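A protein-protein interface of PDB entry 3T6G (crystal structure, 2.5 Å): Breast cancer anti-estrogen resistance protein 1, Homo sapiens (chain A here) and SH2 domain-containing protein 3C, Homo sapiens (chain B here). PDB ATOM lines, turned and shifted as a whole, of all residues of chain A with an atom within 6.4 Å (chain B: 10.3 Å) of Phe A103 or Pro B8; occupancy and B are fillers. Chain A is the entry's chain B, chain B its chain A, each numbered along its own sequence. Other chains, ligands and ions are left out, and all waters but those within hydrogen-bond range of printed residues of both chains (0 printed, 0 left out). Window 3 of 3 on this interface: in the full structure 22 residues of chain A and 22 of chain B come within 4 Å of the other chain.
O of Gln B75 lies within hydrogen-bond range of N of Val B80 (3.5 Å).
NE2 of Gln A107 is in hydrogen-bond range of OE1 of Glu A106 (2.9 Å).
The side-chain sulfur (SG) of Cys A108 sits close to the backbone carbonyl oxygen (O) of Tyr A104 (3.5 Å).
The backbone carbonyl oxygen of Met B78 is in hydrogen-bond range of a ring nitrogen (NE2) of His B91, 2.9 Å away.
OG1 of Thr B6 touches OE1 of Gln A99, at 3.7 Å.
Gln A99 touches Val B7 (OE1 to CG2, 3.1 Å).
CE1 of Phe A103 touches O of Pro B8, 3.8 Å away.
Phe A103 touches His B91.
CG1 of Val B80 touches OH of Tyr A104, 3.999 Å away.
Tyr A104 touches His B91.
Gln A107 touches Pro B90.
His B91 touches Gln A107 (N to OE1, 3.6 Å).
No residue of chain B comes within 4 Å of Leu A102.
Of the printed residues of chain B, Phe A103 touches Pro B8 (3.8 Å) and His B91 (3.99 Å).
Printed residues of chain A within 4 Å of Val B80: Tyr A104 (3.999 Å).
Of the printed residues of chain A, His B91 touches Phe A103, Tyr A104 and Gln A107.
The nearest printed residue of chain B that does not touch Phe A103 is Val B10 (4.2 Å).
The nearest residue of chain A that does not touch Pro B8 is Leu A100 (4.5 Å).
Of the 22 printed residues of chain B, 6 touch a printed residue of chain A.
Printed residues of chain B that touch a printed residue of chain A: Thr B6, Val B7, Pro B8, Val B80, Pro B90 and His B91.
Hydrophobic or aromatic side chains of chain B that line the printed part of chain A: Val B7, Val B80, Pro B90 and His B91.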
ATOM      1  N   ARG A  98      -7.621  15.440 -13.058  1.00  0.00           N
ATOM      2  CA  ARG A  98      -7.150  14.997 -14.370  1.00  0.00           C
ATOM      3  C   ARG A  98      -5.639  14.762 -14.389  1.00  0.00           C
ATOM      4  O   ARG A  98      -5.171  13.756 -14.920  1.00  0.00           O
ATOM      5  CB  ARG A  98      -7.549  15.966 -15.479  1.00  0.00           C
ATOM      6  CG  ARG A  98      -7.126  15.471 -16.853  1.00  0.00           C
ATOM      7  CD  ARG A  98      -7.682  16.316 -17.988  1.00  0.00           C
ATOM      8  NE  ARG A  98      -7.756  15.536 -19.222  1.00  0.00           N
ATOM      9  CZ  ARG A  98      -6.773  15.436 -20.111  1.00  0.00           C
ATOM     10  NH1 ARG A  98      -5.631  16.080 -19.914  1.00  0.00           N
ATOM     11  NH2 ARG A  98      -6.935  14.699 -21.203  1.00  0.00           N
ATOM     12  N   GLN A  99      -4.882  15.692 -13.812  1.00  0.00           N
ATOM     13  CA  GLN A  99      -3.438  15.526 -13.668  1.00  0.00           C
ATOM     14  C   GLN A  99      -3.147  14.188 -13.013  1.00  0.00           C
ATOM     15  O   GLN A  99      -2.282  13.437 -13.453  1.00  0.00           O
ATOM     16  CB  GLN A  99      -2.859  16.633 -12.786  1.00  0.00           C
ATOM     17  CG  GLN A  99      -3.083  18.052 -13.304  1.00  0.00           C
ATOM     18  CD  GLN A  99      -2.153  18.413 -14.451  1.00  0.00           C
ATOM     19  OE1 GLN A  99      -1.472  19.444 -14.414  1.00  0.00           O
ATOM     20  NE2 GLN A  99      -2.120  17.562 -15.479  1.00  0.00           N
ATOM     21  N   LEU A 100      -3.880  13.914 -11.942  1.00  0.00           N
ATOM     22  CA  LEU A 100      -3.689  12.716 -11.155  1.00  0.00           C
ATOM     23  C   LEU A 100      -3.989  11.492 -11.997  1.00  0.00           C
ATOM     24  O   LEU A 100      -3.102  10.673 -12.265  1.00  0.00           O
ATOM     25  CB  LEU A 100      -4.639  12.745  -9.968  1.00  0.00           C
ATOM     26  CG  LEU A 100      -4.040  12.379  -8.620  1.00  0.00           C
ATOM     27  CD1 LEU A 100      -2.771  13.177  -8.346  1.00  0.00           C
ATOM     28  CD2 LEU A 100      -5.082  12.603  -7.539  1.00  0.00           C
ATOM     29  N   LEU A 101      -5.250  11.379 -12.408  1.00  0.00           N
ATOM     30  CA  LEU A 101      -5.701  10.243 -13.198  1.00  0.00           C
ATOM     31  C   LEU A 101      -4.698   9.940 -14.291  1.00  0.00           C
ATOM     32  O   LEU A 101      -4.272   8.805 -14.432  1.00  0.00           O
ATOM     33  CB  LEU A 101      -7.085  10.494 -13.784  1.00  0.00           C
ATOM     34  CG  LEU A 101      -8.225  10.526 -12.767  1.00  0.00           C
ATOM     35  CD1 LEU A 101      -9.540  10.933 -13.441  1.00  0.00           C
ATOM     36  CD2 LEU A 101      -8.353   9.178 -12.058  1.00  0.00           C
ATOM     37  N   LEU A 102      -4.283  10.945 -15.054  1.00  0.00           N
ATOM     38  CA  LEU A 102      -3.301  10.650 -16.095  1.00  0.00           C
ATOM     39  C   LEU A 102      -2.003  10.078 -15.514  1.00  0.00           C
ATOM     40  O   LEU A 102      -1.411   9.159 -16.086  1.00  0.00           O
ATOM     41  CB  LEU A 102      -3.009  11.863 -16.962  1.00  0.00           C
ATOM     42  CG  LEU A 102      -4.152  12.396 -17.825  1.00  0.00           C
ATOM     43  CD1 LEU A 102      -3.606  13.342 -18.911  1.00  0.00           C
ATOM     44  CD2 LEU A 102      -4.948  11.257 -18.438  1.00  0.00           C
ATOM     45  N   PHE A 103      -1.573  10.611 -14.374  1.00  0.00           N
ATOM     46  CA  PHE A 103      -0.310  10.195 -13.776  1.00  0.00           C
ATOM     47  C   PHE A 103      -0.393   8.738 -13.357  1.00  0.00           C
ATOM     48  O   PHE A 103       0.434   7.913 -13.759  1.00  0.00           O
ATOM     49  CB  PHE A 103       0.067  11.083 -12.581  1.00  0.00           C
ATOM     50  CG  PHE A 103       1.261  10.584 -11.813  1.00  0.00           C
ATOM     51  CD1 PHE A 103       2.546  10.842 -12.260  1.00  0.00           C
ATOM     52  CD2 PHE A 103       1.095   9.840 -10.647  1.00  0.00           C
ATOM     53  CE1 PHE A 103       3.641  10.362 -11.561  1.00  0.00           C
ATOM     54  CE2 PHE A 103       2.180   9.366  -9.945  1.00  0.00           C
ATOM     55  CZ  PHE A 103       3.454   9.622 -10.403  1.00  0.00           C
ATOM     56  N   TYR A 104      -1.407   8.416 -12.568  1.00  0.00           N
ATOM     57  CA  TYR A 104      -1.576   7.050 -12.108  1.00  0.00           C
ATOM     58  C   TYR A 104      -2.015   6.071 -13.180  1.00  0.00           C
ATOM     59  O   TYR A 104      -1.628   4.899 -13.140  1.00  0.00           O
ATOM     60  CB  TYR A 104      -2.509   7.002 -10.910  1.00  0.00           C
ATOM     61  CG  TYR A 104      -1.803   7.517  -9.693  1.00  0.00           C
ATOM     62  CD1 TYR A 104      -0.774   6.787  -9.123  1.00  0.00           C
ATOM     63  CD2 TYR A 104      -2.118   8.756  -9.144  1.00  0.00           C
ATOM     64  CE1 TYR A 104      -0.100   7.254  -8.027  1.00  0.00           C
ATOM     65  CE2 TYR A 104      -1.451   9.227  -8.043  1.00  0.00           C
ATOM     66  CZ  TYR A 104      -0.438   8.475  -7.490  1.00  0.00           C
ATOM     67  OH  TYR A 104       0.245   8.927  -6.386  1.00  0.00           O
ATOM     68  N   LEU A 105      -2.828   6.528 -14.131  1.00  0.00           N
ATOM     69  CA  LEU A 105      -3.210   5.670 -15.252  1.00  0.00           C
ATOM     70  C   LEU A 105      -1.926   5.219 -15.944  1.00  0.00           C
ATOM     71  O   LEU A 105      -1.759   4.053 -16.299  1.00  0.00           O
ATOM     72  CB  LEU A 105      -4.103   6.424 -16.238  1.00  0.00           C
ATOM     73  CG  LEU A 105      -4.572   5.632 -17.447  1.00  0.00           C
ATOM     74  CD1 LEU A 105      -5.534   4.557 -16.957  1.00  0.00           C
ATOM     75  CD2 LEU A 105      -5.247   6.531 -18.465  1.00  0.00           C
ATOM     76  N   GLU A 106      -1.004   6.162 -16.089  1.00  0.00           N
ATOM     77  CA  GLU A 106       0.311   5.900 -16.650  1.00  0.00           C
ATOM     78  C   GLU A 106       1.122   4.941 -15.734  1.00  0.00           C
ATOM     79  O   GLU A 106       1.795   4.026 -16.224  1.00  0.00           O
ATOM     80  CB  GLU A 106       1.018   7.240 -16.907  1.00  0.00           C
ATOM     81  CG  GLU A 106       2.451   7.112 -17.314  1.00  0.00           C
ATOM     82  CD  GLU A 106       3.282   6.570 -16.172  1.00  0.00           C
ATOM     83  OE1 GLU A 106       3.196   7.140 -15.056  1.00  0.00           O
ATOM     84  OE2 GLU A 106       4.003   5.569 -16.379  1.00  0.00           O
ATOM     85  N   GLN A 107       1.039   5.136 -14.413  1.00  0.00           N
ATOM     86  CA  GLN A 107       1.692   4.233 -13.463  1.00  0.00           C
ATOM     87  C   GLN A 107       1.107   2.830 -13.580  1.00  0.00           C
ATOM     88  O   GLN A 107       1.837   1.861 -13.766  1.00  0.00           O
ATOM     89  CB  GLN A 107       1.550   4.733 -12.021  1.00  0.00           C
ATOM     90  CG  GLN A 107       2.298   6.019 -11.703  1.00  0.00           C
ATOM     91  CD  GLN A 107       3.808   5.829 -11.633  1.00  0.00           C
ATOM     92  OE1 GLN A 107       4.315   5.157 -10.729  1.00  0.00           O
ATOM     93  NE2 GLN A 107       4.534   6.435 -12.580  1.00  0.00           N
ATOM     94  N   CYS A 108      -0.212   2.723 -13.449  1.00  0.00           N
ATOM     95  CA  CYS A 108      -0.893   1.453 -13.658  1.00  0.00           C
ATOM     96  C   CYS A 108      -0.332   0.779 -14.886  1.00  0.00           C
ATOM     97  O   CYS A 108       0.045  -0.396 -14.860  1.00  0.00           O
ATOM     98  CB  CYS A 108      -2.384   1.661 -13.915  1.00  0.00           C
ATOM     99  SG  CYS A 108      -3.366   1.975 -12.448  1.00  0.00           S
ATOM    100  N   THR B   6       4.183  16.319 -15.476  1.00  0.00           N
ATOM    101  CA  THR B   6       4.116  17.586 -14.755  1.00  0.00           C
ATOM    102  C   THR B   6       3.972  17.406 -13.233  1.00  0.00           C
ATOM    103  O   THR B   6       4.964  17.255 -12.500  1.00  0.00           O
ATOM    104  CB  THR B   6       2.932  18.431 -15.256  1.00  0.00           C
ATOM    105  OG1 THR B   6       1.710  17.717 -15.034  1.00  0.00           O
ATOM    106  CG2 THR B   6       3.071  18.728 -16.757  1.00  0.00           C
ATOM    107  N   VAL B   7       2.716  17.396 -12.785  1.00  0.00           N
ATOM    108  CA  VAL B   7       2.356  17.548 -11.372  1.00  0.00           C
ATOM    109  C   VAL B   7       3.262  16.815 -10.402  1.00  0.00           C
ATOM    110  O   VAL B   7       4.169  17.457  -9.849  1.00  0.00           O
ATOM    111  CB  VAL B   7       0.864  17.234 -11.100  1.00  0.00           C
ATOM    112  CG1 VAL B   7       0.506  17.603  -9.668  1.00  0.00           C
ATOM    113  CG2 VAL B   7      -0.027  17.991 -12.076  1.00  0.00           C
ATOM    114  N   PRO B   8       3.012  15.494 -10.169  1.00  0.00           N
ATOM    115  CA  PRO B   8       3.838  14.660  -9.275  1.00  0.00           C
ATOM    116  C   PRO B   8       5.039  14.097 -10.017  1.00  0.00           C
ATOM    117  O   PRO B   8       4.955  13.860 -11.229  1.00  0.00           O
ATOM    118  CB  PRO B   8       2.898  13.511  -8.853  1.00  0.00           C
ATOM    119  CG  PRO B   8       1.553  13.839  -9.433  1.00  0.00           C
ATOM    120  CD  PRO B   8       1.823  14.756 -10.616  1.00  0.00           C
ATOM    121  N   ILE B   9       6.140  13.892  -9.300  1.00  0.00           N
ATOM    122  CA  ILE B   9       7.396  13.470  -9.913  1.00  0.00           C
ATOM    123  C   ILE B   9       7.830  12.080  -9.468  1.00  0.00           C
ATOM    124  O   ILE B   9       7.222  11.473  -8.589  1.00  0.00           O
ATOM    125  CB  ILE B   9       8.547  14.409  -9.555  1.00  0.00           C
ATOM    126  CG1 ILE B   9       8.827  14.331  -8.045  1.00  0.00           C
ATOM    127  CG2 ILE B   9       8.263  15.835 -10.045  1.00  0.00           C
ATOM    128  CD1 ILE B   9      10.197  14.827  -7.683  1.00  0.00           C
ATOM    129  N   VAL B  10       8.905  11.591 -10.073  1.00  0.00           N
ATOM    130  CA  VAL B  10       9.404  10.255  -9.766  1.00  0.00           C
ATOM    131  C   VAL B  10      10.875  10.354  -9.447  1.00  0.00           C
ATOM    132  O   VAL B  10      11.717  10.539 -10.328  1.00  0.00           O
ATOM    133  CB  VAL B  10       9.171   9.224 -10.921  1.00  0.00           C
ATOM    134  CG1 VAL B  10       9.509   7.804 -10.438  1.00  0.00           C
ATOM    135  CG2 VAL B  10       7.723   9.287 -11.423  1.00  0.00           C
ATOM    136  N   GLU B  11      11.174  10.262  -8.165  1.00  0.00           N
ATOM    137  CA  GLU B  11      12.543  10.301  -7.708  1.00  0.00           C
ATOM    138  C   GLU B  11      13.289   9.144  -8.341  1.00  0.00           C
ATOM    139  O   GLU B  11      12.872   7.997  -8.248  1.00  0.00           O
ATOM    140  CB  GLU B  11      12.548  10.226  -6.190  1.00  0.00           C
ATOM    141  CG  GLU B  11      11.610  11.268  -5.607  1.00  0.00           C
ATOM    142  CD  GLU B  11      11.505  11.213  -4.105  1.00  0.00           C
ATOM    143  OE1 GLU B  11      12.291  10.464  -3.483  1.00  0.00           O
ATOM    144  OE2 GLU B  11      10.631  11.928  -3.560  1.00  0.00           O
ATOM    145  N   LYS B  72       4.040  21.253   2.340  1.00  0.00           N
ATOM    146  CA  LYS B  72       3.040  21.051   1.287  1.00  0.00           C
ATOM    147  C   LYS B  72       3.721  20.976  -0.063  1.00  0.00           C
ATOM    148  O   LYS B  72       3.260  20.277  -0.962  1.00  0.00           O
ATOM    149  CB  LYS B  72       1.949  22.124   1.296  1.00  0.00           C
ATOM    150  CG  LYS B  72       0.933  21.912   2.417  1.00  0.00           C
ATOM    151  CD  LYS B  72       1.634  21.716   3.783  1.00  0.00           C
ATOM    152  CE  LYS B  72       0.703  21.147   4.863  1.00  0.00           C
ATOM    153  NZ  LYS B  72       0.466  19.678   4.725  1.00  0.00           N
ATOM    154  N   GLU B  73       4.837  21.672  -0.211  1.00  0.00           N
ATOM    155  CA  GLU B  73       5.552  21.567  -1.463  1.00  0.00           C
ATOM    156  C   GLU B  73       6.154  20.174  -1.639  1.00  0.00           C
ATOM    157  O   GLU B  73       6.262  19.696  -2.765  1.00  0.00           O
ATOM    158  CB  GLU B  73       6.588  22.664  -1.621  1.00  0.00           C
ATOM    159  CG  GLU B  73       5.975  24.051  -1.705  1.00  0.00           C
ATOM    160  CD  GLU B  73       5.717  24.684  -0.337  1.00  0.00           C
ATOM    161  OE1 GLU B  73       6.046  24.087   0.712  1.00  0.00           O
ATOM    162  OE2 GLU B  73       5.186  25.800  -0.306  1.00  0.00           O
ATOM    163  N   MET B  74       6.535  19.519  -0.541  1.00  0.00           N
ATOM    164  CA  MET B  74       7.020  18.143  -0.611  1.00  0.00           C
ATOM    165  C   MET B  74       5.870  17.228  -1.044  1.00  0.00           C
ATOM    166  O   MET B  74       6.044  16.353  -1.895  1.00  0.00           O
ATOM    167  CB  MET B  74       7.601  17.685   0.736  1.00  0.00           C
ATOM    168  CG  MET B  74       8.930  18.350   1.139  1.00  0.00           C
ATOM    169  SD  MET B  74       9.391  18.105   2.878  1.00  0.00           S
ATOM    170  CE  MET B  74       9.404  16.296   2.972  1.00  0.00           C
ATOM    171  N   GLN B  75       4.698  17.451  -0.457  1.00  0.00           N
ATOM    172  CA  GLN B  75       3.499  16.682  -0.756  1.00  0.00           C
ATOM    173  C   GLN B  75       3.071  16.763  -2.230  1.00  0.00           C
ATOM    174  O   GLN B  75       2.579  15.797  -2.826  1.00  0.00           O
ATOM    175  CB  GLN B  75       2.359  17.158   0.150  1.00  0.00           C
ATOM    176  CG  GLN B  75       2.440  16.569   1.572  1.00  0.00           C
ATOM    177  CD  GLN B  75       1.554  17.293   2.575  1.00  0.00           C
ATOM    178  OE1 GLN B  75       1.039  18.376   2.294  1.00  0.00           O
ATOM    179  NE2 GLN B  75       1.383  16.703   3.757  1.00  0.00           N
ATOM    180  N   THR B  76       3.242  17.931  -2.815  1.00  0.00           N
ATOM    181  CA  THR B  76       2.791  18.146  -4.168  1.00  0.00           C
ATOM    182  C   THR B  76       3.695  17.350  -5.088  1.00  0.00           C
ATOM    183  O   THR B  76       3.234  16.751  -6.055  1.00  0.00           O
ATOM    184  CB  THR B  76       2.819  19.660  -4.529  1.00  0.00           C
ATOM    185  OG1 THR B  76       1.773  20.329  -3.815  1.00  0.00           O
ATOM    186  CG2 THR B  76       2.628  19.864  -6.009  1.00  0.00           C
ATOM    187  N   LEU B  77       4.986  17.343  -4.787  1.00  0.00           N
ATOM    188  CA  LEU B  77       5.930  16.616  -5.619  1.00  0.00           C
ATOM    189  C   LEU B  77       5.709  15.110  -5.486  1.00  0.00           C
ATOM    190  O   LEU B  77       5.978  14.371  -6.419  1.00  0.00           O
ATOM    191  CB  LEU B  77       7.381  16.959  -5.260  1.00  0.00           C
ATOM    192  CG  LEU B  77       7.864  18.415  -5.266  1.00  0.00           C
ATOM    193  CD1 LEU B  77       9.311  18.472  -4.808  1.00  0.00           C
ATOM    194  CD2 LEU B  77       7.686  19.100  -6.630  1.00  0.00           C
ATOM    195  N   MET B  78       5.237  14.664  -4.321  1.00  0.00           N
ATOM    196  CA  MET B  78       5.072  13.233  -4.052  1.00  0.00           C
ATOM    197  C   MET B  78       3.774  12.748  -4.655  1.00  0.00           C
ATOM    198  O   MET B  78       3.677  11.599  -5.075  1.00  0.00           O
ATOM    199  CB  MET B  78       5.013  12.929  -2.540  1.00  0.00           C
ATOM    200  CG  MET B  78       6.242  13.257  -1.764  1.00  0.00           C
ATOM    201  SD  MET B  78       6.377  12.380  -0.199  1.00  0.00           S
ATOM    202  CE  MET B  78       5.018  12.962   0.798  1.00  0.00           C
ATOM    203  N   GLY B  79       2.773  13.630  -4.666  1.00  0.00           N
ATOM    204  CA  GLY B  79       1.415  13.277  -5.056  1.00  0.00           C
ATOM    205  C   GLY B  79       0.583  12.827  -3.862  1.00  0.00           C
ATOM    206  O   GLY B  79      -0.645  12.713  -3.967  1.00  0.00           O
ATOM    207  N   VAL B  80       1.249  12.584  -2.723  1.00  0.00           N
ATOM    208  CA  VAL B  80       0.569  12.106  -1.521  1.00  0.00           C
ATOM    209  C   VAL B  80       1.005  12.895  -0.292  1.00  0.00           C
ATOM    210  O   VAL B  80       2.068  13.516  -0.294  1.00  0.00           O
ATOM    211  CB  VAL B  80       0.847  10.603  -1.286  1.00  0.00           C
ATOM    212  CG1 VAL B  80       0.412   9.798  -2.487  1.00  0.00           C
ATOM    213  CG2 VAL B  80       2.307  10.365  -1.060  1.00  0.00           C
ATOM    214  N   ARG B  81       0.180  12.884   0.752  1.00  0.00           N
ATOM    215  CA  ARG B  81       0.533  13.568   1.992  1.00  0.00           C
ATOM    216  C   ARG B  81       1.741  12.969   2.733  1.00  0.00           C
ATOM    217  O   ARG B  81       2.623  13.703   3.159  1.00  0.00           O
ATOM    218  CB  ARG B  81      -0.673  13.633   2.931  1.00  0.00           C
ATOM    219  CG  ARG B  81      -1.669  14.709   2.564  1.00  0.00           C
ATOM    220  CD  ARG B  81      -2.850  14.746   3.523  1.00  0.00           C
ATOM    221  NE  ARG B  81      -3.596  16.001   3.404  1.00  0.00           N
ATOM    222  CZ  ARG B  81      -4.366  16.338   2.366  1.00  0.00           C
ATOM    223  NH1 ARG B  81      -4.503  15.517   1.328  1.00  0.00           N
ATOM    224  NH2 ARG B  81      -4.999  17.507   2.364  1.00  0.00           N
ATOM    225  N   LEU B  86       3.442   6.999   0.312  1.00  0.00           N
ATOM    226  CA  LEU B  86       4.346   6.996  -0.831  1.00  0.00           C
ATOM    227  C   LEU B  86       5.009   5.644  -1.062  1.00  0.00           C
ATOM    228  O   LEU B  86       5.246   5.259  -2.203  1.00  0.00           O
ATOM    229  CB  LEU B  86       5.416   8.093  -0.718  1.00  0.00           C
ATOM    230  CG  LEU B  86       6.341   8.093  -1.945  1.00  0.00           C
ATOM    231  CD1 LEU B  86       5.520   8.381  -3.206  1.00  0.00           C
ATOM    232  CD2 LEU B  86       7.507   9.070  -1.857  1.00  0.00           C
ATOM    233  N   LEU B  89       3.294   2.997  -3.333  1.00  0.00           N
ATOM    234  CA  LEU B  89       3.108   3.384  -4.725  1.00  0.00           C
ATOM    235  C   LEU B  89       4.325   3.063  -5.587  1.00  0.00           C
ATOM    236  O   LEU B  89       5.430   2.939  -5.086  1.00  0.00           O
ATOM    237  CB  LEU B  89       2.764   4.872  -4.827  1.00  0.00           C
ATOM    238  CG  LEU B  89       1.317   5.207  -4.499  1.00  0.00           C
ATOM    239  CD1 LEU B  89       0.529   3.934  -4.437  1.00  0.00           C
ATOM    240  CD2 LEU B  89       1.222   5.943  -3.189  1.00  0.00           C
ATOM    241  N   PRO B  90       4.130   2.936  -6.906  1.00  0.00           N
ATOM    242  CA  PRO B  90       5.230   2.341  -7.658  1.00  0.00           C
ATOM    243  C   PRO B  90       6.378   3.326  -7.731  1.00  0.00           C
ATOM    244  O   PRO B  90       7.526   2.915  -7.897  1.00  0.00           O
ATOM    245  CB  PRO B  90       4.626   2.114  -9.052  1.00  0.00           C
ATOM    246  CG  PRO B  90       3.186   2.556  -8.950  1.00  0.00           C
ATOM    247  CD  PRO B  90       3.111   3.498  -7.799  1.00  0.00           C
ATOM    248  N   HIS B  91       6.075   4.615  -7.620  1.00  0.00           N
ATOM    249  CA  HIS B  91       7.130   5.621  -7.696  1.00  0.00           C
ATOM    250  C   HIS B  91       7.784   5.858  -6.340  1.00  0.00           C
ATOM    251  O   HIS B  91       8.815   6.500  -6.255  1.00  0.00           O
ATOM    252  CB  HIS B  91       6.665   6.941  -8.342  1.00  0.00           C
ATOM    253  CG  HIS B  91       5.652   7.708  -7.548  1.00  0.00           C
ATOM    254  ND1 HIS B  91       4.441   7.175  -7.158  1.00  0.00           N
ATOM    255  CD2 HIS B  91       5.650   8.994  -7.113  1.00  0.00           C
ATOM    256  CE1 HIS B  91       3.744   8.087  -6.503  1.00  0.00           C
ATOM    257  NE2 HIS B  91       4.458   9.199  -6.460  1.00  0.00           N
ATOM    258  N   GLY B  92       7.173   5.321  -5.292  1.00  0.00           N
ATOM    259  CA  GLY B  92       7.781   5.274  -3.977  1.00  0.00           C
ATOM    260  C   GLY B  92       9.023   4.399  -3.965  1.00  0.00           C
ATOM    261  O   GLY B  92       9.598   4.132  -2.920  1.00  0.00           O
ATOM    262  N   ARG B  93       9.457   3.958  -5.134  1.00  0.00           N
ATOM    263  CA  ARG B  93      10.596   3.047  -5.201  1.00  0.00           C
ATOM    264  C   ARG B  93      11.871   3.599  -4.527  1.00  0.00           C
ATOM    265  O   ARG B  93      12.549   2.891  -3.781  1.00  0.00           O
ATOM    266  CB  ARG B  93      10.856   2.627  -6.655  1.00  0.00           C
ATOM    267  CG  ARG B  93      12.261   2.117  -6.932  1.00  0.00           C
ATOM    268  CD  ARG B  93      12.295   1.147  -8.117  1.00  0.00           C
ATOM    269  NE  ARG B  93      12.866  -0.141  -7.731  1.00  0.00           N
ATOM    270  CZ  ARG B  93      14.136  -0.485  -7.932  1.00  0.00           C
ATOM    271  NH1 ARG B  93      14.971   0.357  -8.541  1.00  0.00           N
ATOM    272  NH2 ARG B  93      14.570  -1.676  -7.528  1.00  0.00           N
